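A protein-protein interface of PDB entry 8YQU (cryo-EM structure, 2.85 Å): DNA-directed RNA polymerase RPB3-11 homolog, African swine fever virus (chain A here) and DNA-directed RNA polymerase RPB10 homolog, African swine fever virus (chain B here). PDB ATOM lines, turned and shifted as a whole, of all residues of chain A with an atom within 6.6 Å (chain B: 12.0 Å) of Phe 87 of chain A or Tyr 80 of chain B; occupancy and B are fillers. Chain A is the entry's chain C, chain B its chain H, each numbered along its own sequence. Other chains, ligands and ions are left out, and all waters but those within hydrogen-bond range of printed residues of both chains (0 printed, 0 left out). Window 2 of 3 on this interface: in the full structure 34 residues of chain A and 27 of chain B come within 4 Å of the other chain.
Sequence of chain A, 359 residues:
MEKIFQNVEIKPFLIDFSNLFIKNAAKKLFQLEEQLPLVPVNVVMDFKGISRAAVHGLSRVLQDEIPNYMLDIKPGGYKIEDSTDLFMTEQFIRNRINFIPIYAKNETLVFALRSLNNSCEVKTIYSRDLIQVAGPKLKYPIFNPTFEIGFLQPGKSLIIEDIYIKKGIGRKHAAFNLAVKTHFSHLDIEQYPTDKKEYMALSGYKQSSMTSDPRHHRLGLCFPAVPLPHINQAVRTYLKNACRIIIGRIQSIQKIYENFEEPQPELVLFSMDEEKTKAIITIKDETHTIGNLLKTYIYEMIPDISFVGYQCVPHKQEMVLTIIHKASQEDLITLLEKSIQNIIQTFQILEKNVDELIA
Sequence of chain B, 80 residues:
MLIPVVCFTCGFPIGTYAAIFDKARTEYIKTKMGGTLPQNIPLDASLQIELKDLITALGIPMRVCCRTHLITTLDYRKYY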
ATOM      1  N   THR A  84       5.550  11.268 -22.894  1.00  0.00           N
ATOM      2  CA  THR A  84       6.591  10.472 -22.260  1.00  0.00           C
ATOM      3  C   THR A  84       6.333   8.973 -22.327  1.00  0.00           C
ATOM      4  O   THR A  84       7.193   8.197 -21.896  1.00  0.00           O
ATOM      5  CB  THR A  84       6.756  10.887 -20.793  1.00  0.00           C
ATOM      6  OG1 THR A  84       5.477  10.889 -20.149  1.00  0.00           O
ATOM      7  CG2 THR A  84       7.368  12.274 -20.699  1.00  0.00           C
ATOM      8  N   ASP A  85       5.185   8.545 -22.847  1.00  0.00           N
ATOM      9  CA  ASP A  85       4.884   7.120 -22.900  1.00  0.00           C
ATOM     10  C   ASP A  85       5.792   6.424 -23.905  1.00  0.00           C
ATOM     11  O   ASP A  85       6.000   6.915 -25.018  1.00  0.00           O
ATOM     12  CB  ASP A  85       3.422   6.892 -23.268  1.00  0.00           C
ATOM     13  CG  ASP A  85       3.013   5.440 -23.130  1.00  0.00           C
ATOM     14  OD1 ASP A  85       2.784   4.993 -21.987  1.00  0.00           O
ATOM     15  OD2 ASP A  85       2.935   4.741 -24.159  1.00  0.00           O
ATOM     16  N   LEU A  86       6.329   5.272 -23.508  1.00  0.00           N
ATOM     17  CA  LEU A  86       7.283   4.546 -24.334  1.00  0.00           C
ATOM     18  C   LEU A  86       6.632   3.546 -25.277  1.00  0.00           C
ATOM     19  O   LEU A  86       7.300   3.059 -26.196  1.00  0.00           O
ATOM     20  CB  LEU A  86       8.290   3.815 -23.444  1.00  0.00           C
ATOM     21  CG  LEU A  86       9.229   4.689 -22.613  1.00  0.00           C
ATOM     22  CD1 LEU A  86      10.211   3.824 -21.841  1.00  0.00           C
ATOM     23  CD2 LEU A  86       9.962   5.684 -23.499  1.00  0.00           C
ATOM     24  N   PHE A  87       5.353   3.228 -25.079  1.00  0.00           N
ATOM     25  CA  PHE A  87       4.677   2.216 -25.880  1.00  0.00           C
ATOM     26  C   PHE A  87       3.672   2.782 -26.868  1.00  0.00           C
ATOM     27  O   PHE A  87       3.462   2.181 -27.922  1.00  0.00           O
ATOM     28  CB  PHE A  87       3.966   1.207 -24.970  1.00  0.00           C
ATOM     29  CG  PHE A  87       4.900   0.427 -24.093  1.00  0.00           C
ATOM     30  CD1 PHE A  87       5.441  -0.769 -24.529  1.00  0.00           C
ATOM     31  CD2 PHE A  87       5.249   0.896 -22.839  1.00  0.00           C
ATOM     32  CE1 PHE A  87       6.305  -1.487 -23.727  1.00  0.00           C
ATOM     33  CE2 PHE A  87       6.114   0.184 -22.034  1.00  0.00           C
ATOM     34  CZ  PHE A  87       6.643  -1.009 -22.480  1.00  0.00           C
ATOM     35  N   MET A  88       3.046   3.918 -26.560  1.00  0.00           N
ATOM     36  CA  MET A  88       2.080   4.536 -27.467  1.00  0.00           C
ATOM     37  C   MET A  88       2.843   5.386 -28.478  1.00  0.00           C
ATOM     38  O   MET A  88       2.966   6.607 -28.357  1.00  0.00           O
ATOM     39  CB  MET A  88       1.057   5.356 -26.695  1.00  0.00           C
ATOM     40  CG  MET A  88       0.131   4.522 -25.830  1.00  0.00           C
ATOM     41  SD  MET A  88      -0.819   3.319 -26.777  1.00  0.00           S
ATOM     42  CE  MET A  88      -0.005   1.795 -26.311  1.00  0.00           C
ATOM     43  N   THR A  89       3.364   4.713 -29.498  1.00  0.00           N
ATOM     44  CA  THR A  89       4.109   5.389 -30.544  1.00  0.00           C
ATOM     45  C   THR A  89       3.164   6.202 -31.426  1.00  0.00           C
ATOM     46  O   THR A  89       1.941   6.046 -31.390  1.00  0.00           O
ATOM     47  CB  THR A  89       4.886   4.379 -31.385  1.00  0.00           C
ATOM     48  OG1 THR A  89       3.973   3.455 -31.987  1.00  0.00           O
ATOM     49  CG2 THR A  89       5.867   3.613 -30.515  1.00  0.00           C
ATOM     50  N   GLU A  90       3.752   7.094 -32.226  1.00  0.00           N
ATOM     51  CA  GLU A  90       2.946   7.929 -33.109  1.00  0.00           C
ATOM     52  C   GLU A  90       2.230   7.094 -34.160  1.00  0.00           C
ATOM     53  O   GLU A  90       1.060   7.347 -34.470  1.00  0.00           O
ATOM     54  CB  GLU A  90       3.818   8.991 -33.778  1.00  0.00           C
ATOM     55  CG  GLU A  90       3.036   9.962 -34.645  1.00  0.00           C
ATOM     56  CD  GLU A  90       3.926  10.953 -35.363  1.00  0.00           C
ATOM     57  OE1 GLU A  90       5.163  10.843 -35.236  1.00  0.00           O
ATOM     58  OE2 GLU A  90       3.388  11.841 -36.057  1.00  0.00           O
ATOM     59  N   PHE A  92       1.223   3.890 -34.054  1.00  0.00           N
ATOM     60  CA  PHE A  92       0.116   3.136 -33.470  1.00  0.00           C
ATOM     61  C   PHE A  92      -1.071   4.043 -33.164  1.00  0.00           C
ATOM     62  O   PHE A  92      -2.214   3.738 -33.528  1.00  0.00           O
ATOM     63  CB  PHE A  92       0.593   2.423 -32.205  1.00  0.00           C
ATOM     64  CG  PHE A  92      -0.431   1.511 -31.594  1.00  0.00           C
ATOM     65  CD1 PHE A  92      -0.757   0.309 -32.198  1.00  0.00           C
ATOM     66  CD2 PHE A  92      -1.064   1.854 -30.412  1.00  0.00           C
ATOM     67  CE1 PHE A  92      -1.698  -0.531 -31.636  1.00  0.00           C
ATOM     68  CE2 PHE A  92      -2.006   1.018 -29.847  1.00  0.00           C
ATOM     69  CZ  PHE A  92      -2.322  -0.175 -30.459  1.00  0.00           C
ATOM     70  N   ILE A  93      -0.813   5.172 -32.502  1.00  0.00           N
ATOM     71  CA  ILE A  93      -1.900   6.051 -32.085  1.00  0.00           C
ATOM     72  C   ILE A  93      -2.592   6.666 -33.294  1.00  0.00           C
ATOM     73  O   ILE A  93      -3.824   6.764 -33.335  1.00  0.00           O
ATOM     74  CB  ILE A  93      -1.375   7.128 -31.121  1.00  0.00           C
ATOM     75  CG1 ILE A  93      -0.914   6.487 -29.814  1.00  0.00           C
ATOM     76  CG2 ILE A  93      -2.454   8.151 -30.838  1.00  0.00           C
ATOM     77  CD1 ILE A  93      -2.021   5.786 -29.066  1.00  0.00           C
ATOM     78  N   VAL A 122      -1.986   1.359 -14.980  1.00  0.00           N
ATOM     79  CA  VAL A 122      -2.129   1.683 -16.394  1.00  0.00           C
ATOM     80  C   VAL A 122      -3.502   2.286 -16.639  1.00  0.00           C
ATOM     81  O   VAL A 122      -4.530   1.706 -16.265  1.00  0.00           O
ATOM     82  CB  VAL A 122      -1.907   0.427 -17.250  1.00  0.00           C
ATOM     83  CG1 VAL A 122      -2.116   0.739 -18.722  1.00  0.00           C
ATOM     84  CG2 VAL A 122      -0.518  -0.138 -17.010  1.00  0.00           C
ATOM     85  N   PHE A 151      -3.324   3.231 -24.092  1.00  0.00           N
ATOM     86  CA  PHE A 151      -3.154   3.063 -22.656  1.00  0.00           C
ATOM     87  C   PHE A 151      -1.791   3.598 -22.244  1.00  0.00           C
ATOM     88  O   PHE A 151      -0.813   3.466 -22.985  1.00  0.00           O
ATOM     89  CB  PHE A 151      -3.305   1.595 -22.230  1.00  0.00           C
ATOM     90  CG  PHE A 151      -2.407   0.647 -22.972  1.00  0.00           C
ATOM     91  CD1 PHE A 151      -2.824   0.060 -24.154  1.00  0.00           C
ATOM     92  CD2 PHE A 151      -1.155   0.325 -22.478  1.00  0.00           C
ATOM     93  CE1 PHE A 151      -2.007  -0.817 -24.835  1.00  0.00           C
ATOM     94  CE2 PHE A 151      -0.333  -0.551 -23.156  1.00  0.00           C
ATOM     95  CZ  PHE A 151      -0.760  -1.124 -24.335  1.00  0.00           C
ATOM     96  N   GLN A 153       1.268   3.799 -19.275  1.00  0.00           N
ATOM     97  CA  GLN A 153       1.909   3.252 -18.096  1.00  0.00           C
ATOM     98  C   GLN A 153       1.889   4.292 -16.979  1.00  0.00           C
ATOM     99  O   GLN A 153       1.728   5.487 -17.239  1.00  0.00           O
ATOM    100  CB  GLN A 153       3.345   2.846 -18.424  1.00  0.00           C
ATOM    101  CG  GLN A 153       3.458   1.803 -19.523  1.00  0.00           C
ATOM    102  CD  GLN A 153       2.852   0.473 -19.128  1.00  0.00           C
ATOM    103  OE1 GLN A 153       3.063  -0.012 -18.017  1.00  0.00           O
ATOM    104  NE2 GLN A 153       2.094  -0.125 -20.039  1.00  0.00           N
ATOM    105  N   MET B   1      -1.895  -4.208 -30.085  1.00  0.00           N
ATOM    106  CA  MET B   1      -1.741  -4.151 -28.637  1.00  0.00           C
ATOM    107  C   MET B   1      -3.100  -4.080 -27.949  1.00  0.00           C
ATOM    108  O   MET B   1      -3.209  -4.300 -26.744  1.00  0.00           O
ATOM    109  CB  MET B   1      -0.874  -2.956 -28.240  1.00  0.00           C
ATOM    110  CG  MET B   1       0.602  -3.144 -28.552  1.00  0.00           C
ATOM    111  SD  MET B   1       1.667  -1.957 -27.715  1.00  0.00           S
ATOM    112  CE  MET B   1       1.553  -0.559 -28.825  1.00  0.00           C
ATOM    113  N   LEU B   2      -4.134  -3.769 -28.727  1.00  0.00           N
ATOM    114  CA  LEU B   2      -5.510  -3.761 -28.251  1.00  0.00           C
ATOM    115  C   LEU B   2      -6.401  -4.340 -29.340  1.00  0.00           C
ATOM    116  O   LEU B   2      -5.946  -4.646 -30.446  1.00  0.00           O
ATOM    117  CB  LEU B   2      -5.975  -2.351 -27.869  1.00  0.00           C
ATOM    118  CG  LEU B   2      -5.129  -1.528 -26.902  1.00  0.00           C
ATOM    119  CD1 LEU B   2      -5.358  -0.045 -27.131  1.00  0.00           C
ATOM    120  CD2 LEU B   2      -5.464  -1.905 -25.473  1.00  0.00           C
ATOM    121  N   LEU B  74      -5.245 -10.244 -28.985  1.00  0.00           N
ATOM    122  CA  LEU B  74      -4.555 -10.151 -27.709  1.00  0.00           C
ATOM    123  C   LEU B  74      -4.514  -8.708 -27.226  1.00  0.00           C
ATOM    124  O   LEU B  74      -4.551  -7.762 -28.017  1.00  0.00           O
ATOM    125  CB  LEU B  74      -3.131 -10.695 -27.824  1.00  0.00           C
ATOM    126  CG  LEU B  74      -2.967 -12.150 -28.263  1.00  0.00           C
ATOM    127  CD1 LEU B  74      -1.495 -12.507 -28.354  1.00  0.00           C
ATOM    128  CD2 LEU B  74      -3.687 -13.083 -27.309  1.00  0.00           C
ATOM    129  N   ASP B  75      -4.430  -8.545 -25.910  1.00  0.00           N
ATOM    130  CA  ASP B  75      -4.354  -7.235 -25.280  1.00  0.00           C
ATOM    131  C   ASP B  75      -2.994  -7.102 -24.608  1.00  0.00           C
ATOM    132  O   ASP B  75      -2.619  -7.945 -23.788  1.00  0.00           O
ATOM    133  CB  ASP B  75      -5.487  -7.055 -24.264  1.00  0.00           C
ATOM    134  CG  ASP B  75      -5.553  -5.650 -23.684  1.00  0.00           C
ATOM    135  OD1 ASP B  75      -4.536  -4.926 -23.693  1.00  0.00           O
ATOM    136  OD2 ASP B  75      -6.642  -5.265 -23.210  1.00  0.00           O
ATOM    137  N   TYR B  76      -2.263  -6.042 -24.958  1.00  0.00           N
ATOM    138  CA  TYR B  76      -0.926  -5.848 -24.408  1.00  0.00           C
ATOM    139  C   TYR B  76      -0.966  -5.522 -22.921  1.00  0.00           C
ATOM    140  O   TYR B  76      -0.018  -5.839 -22.194  1.00  0.00           O
ATOM    141  CB  TYR B  76      -0.206  -4.739 -25.173  1.00  0.00           C
ATOM    142  CG  TYR B  76       1.297  -4.733 -25.013  1.00  0.00           C
ATOM    143  CD1 TYR B  76       2.103  -5.530 -25.812  1.00  0.00           C
ATOM    144  CD2 TYR B  76       1.910  -3.917 -24.074  1.00  0.00           C
ATOM    145  CE1 TYR B  76       3.477  -5.522 -25.674  1.00  0.00           C
ATOM    146  CE2 TYR B  76       3.282  -3.902 -23.929  1.00  0.00           C
ATOM    147  CZ  TYR B  76       4.060  -4.706 -24.731  1.00  0.00           C
ATOM    148  OH  TYR B  76       5.427  -4.694 -24.590  1.00  0.00           O
ATOM    149  N   ARG B  77      -2.043  -4.887 -22.452  1.00  0.00           N
ATOM    150  CA  ARG B  77      -2.142  -4.542 -21.038  1.00  0.00           C
ATOM    151  C   ARG B  77      -2.203  -5.781 -20.159  1.00  0.00           C
ATOM    152  O   ARG B  77      -1.795  -5.737 -18.993  1.00  0.00           O
ATOM    153  CB  ARG B  77      -3.376  -3.676 -20.790  1.00  0.00           C
ATOM    154  CG  ARG B  77      -3.390  -2.368 -21.550  1.00  0.00           C
ATOM    155  CD  ARG B  77      -4.750  -1.699 -21.452  1.00  0.00           C
ATOM    156  NE  ARG B  77      -5.777  -2.446 -22.167  1.00  0.00           N
ATOM    157  CZ  ARG B  77      -7.051  -2.088 -22.240  1.00  0.00           C
ATOM    158  NH1 ARG B  77      -7.492  -0.985 -21.657  1.00  0.00           N
ATOM    159  NH2 ARG B  77      -7.903  -2.852 -22.916  1.00  0.00           N
ATOM    160  N   LYS B  78      -2.708  -6.890 -20.694  1.00  0.00           N
ATOM    161  CA  LYS B  78      -2.927  -8.097 -19.912  1.00  0.00           C
ATOM    162  C   LYS B  78      -1.712  -9.010 -19.862  1.00  0.00           C
ATOM    163  O   LYS B  78      -1.724  -9.989 -19.109  1.00  0.00           O
ATOM    164  CB  LYS B  78      -4.129  -8.860 -20.474  1.00  0.00           C
ATOM    165  CG  LYS B  78      -5.435  -8.095 -20.343  1.00  0.00           C
ATOM    166  CD  LYS B  78      -6.589  -8.830 -20.994  1.00  0.00           C
ATOM    167  CE  LYS B  78      -7.898  -8.095 -20.765  1.00  0.00           C
ATOM    168  NZ  LYS B  78      -9.049  -8.806 -21.383  1.00  0.00           N
ATOM    169  N   TYR B  79      -0.666  -8.716 -20.637  1.00  0.00           N
ATOM    170  CA  TYR B  79       0.572  -9.476 -20.592  1.00  0.00           C
ATOM    171  C   TYR B  79       1.755  -8.678 -20.071  1.00  0.00           C
ATOM    172  O   TYR B  79       2.776  -9.281 -19.720  1.00  0.00           O
ATOM    173  CB  TYR B  79       0.922 -10.024 -21.985  1.00  0.00           C
ATOM    174  CG  TYR B  79      -0.088 -11.000 -22.535  1.00  0.00           C
ATOM    175  CD1 TYR B  79      -0.084 -12.329 -22.137  1.00  0.00           C
ATOM    176  CD2 TYR B  79      -1.043 -10.596 -23.455  1.00  0.00           C
ATOM    177  CE1 TYR B  79      -1.005 -13.226 -22.638  1.00  0.00           C
ATOM    178  CE2 TYR B  79      -1.968 -11.485 -23.961  1.00  0.00           C
ATOM    179  CZ  TYR B  79      -1.944 -12.799 -23.550  1.00  0.00           C
ATOM    180  OH  TYR B  79      -2.864 -13.689 -24.053  1.00  0.00           O
ATOM    181  N   TYR B  80       1.654  -7.355 -20.009  1.00  0.00           N
ATOM    182  CA  TYR B  80       2.766  -6.523 -19.573  1.00  0.00           C
ATOM    183  C   TYR B  80       2.414  -5.756 -18.304  1.00  0.00           C
ATOM    184  O   TYR B  80       1.797  -4.693 -18.361  1.00  0.00           O
ATOM    185  CB  TYR B  80       3.165  -5.550 -20.683  1.00  0.00           C
ATOM    186  CG  TYR B  80       4.397  -4.735 -20.372  1.00  0.00           C
ATOM    187  CD1 TYR B  80       5.661  -5.302 -20.440  1.00  0.00           C
ATOM    188  CD2 TYR B  80       4.297  -3.400 -20.011  1.00  0.00           C
ATOM    189  CE1 TYR B  80       6.789  -4.563 -20.158  1.00  0.00           C
ATOM    190  CE2 TYR B  80       5.422  -2.653 -19.726  1.00  0.00           C
ATOM    191  CZ  TYR B  80       6.665  -3.240 -19.804  1.00  0.00           C
ATOM    192  OH  TYR B  80       7.789  -2.501 -19.520  1.00  0.00           O
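OD2 of Asp 85 of chain A lies within hydrogen-bond range of N of Phe 87 of chain A (3.0 Å).
The side-chain carboxylate (OD2) of Asp 85 of chain A is in hydrogen-bond range of the backbone NH (N) of Met 88 of chain A (2.5 Å).
OD1 of Asp 85 of chain A sits at hydrogen-bond distance from N of Gln 153 of chain A, at 3.3 Å.
N of Phe 151 of chain A lies within hydrogen-bond range of SD of Met 88 of chain A (3.7 Å).
OG1 of Thr 89 of chain A lies within hydrogen-bond range of N of Phe 92 of chain A (3.5 Å).
The side-chain carboxylate of Asp 75 of chain B lies within salt-bridge range of the guanidinium group of Arg 77 of chain B (2.7 Å).
O of Phe 87 of chain A touches CE of Met 1 of chain B, 3.5 Å away.
Tyr 76 of chain B touches Phe 87 of chain A (OH to CE1, 3.4 Å).
Phe 87 of chain A touches Tyr 80 of chain B.
Met 1 of chain B touches Met 88 of chain A.
CZ of Phe 92 of chain A touches CB of Met 1 of chain B (3.8 Å).
Phe 151 of chain A touches Leu 2 of chain B (CD1 to CD2, 3.5 Å).
Phe 151 of chain A touches Tyr 76 of chain B.
Arg 77 of chain B touches Phe 151 of chain A.
CE2 of Tyr 80 of chain B touches OE1 of Gln 153 of chain A, at 3.9 Å.
Of the printed residues of chain A, Tyr 80 of chain B touches Phe 87 (3.4 Å) and Gln 153 (3.9 Å).
No residue of chain B comes within 4 Å of Asp 85 of chain A.
Leu 86 of chain A touches none of the printed residues of chain B.
Of chain B, only Met 1 (3.8 Å) comes within 4 Å of Met 88 of chain A.
No residue of chain B comes within 4 Å of Thr 89 of chain A.
Phe 151 of chain A touches just these residues of chain B: Leu 2 (3.5 Å), Tyr 76 (3.8 Å) and Arg 77 (3.5 Å).
Printed residues of chain A within 4 Å of Arg 77 of chain B: Phe 151 (3.5 Å).
Printed residues of chain B within 4 Å of Phe 92 of chain A: Met 1 (3.8 Å).
Of the printed residues of chain A, Met 1 of chain B touches Phe 87, Met 88 and Phe 92.
Of the printed residues of chain A, Leu 2 of chain B touches Phe 151.
The nearest residue of chain A that does not touch Tyr 80 of chain B is Val 122 of chain A (5.3 Å).
Of the 9 printed residues of chain B, 5 touch a printed residue of chain A.
Printed residues of chain B that touch a printed residue of chain A: Met 1, Leu 2, Tyr 76, Arg 77 and Tyr 80.
Hydrophobic or aromatic side chains of chain A within 4 Å of the printed part of chain B: Phe 87, Met 88, Phe 92 and Phe 151.
Among the printed residues, 9 pairs touch across the chains.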
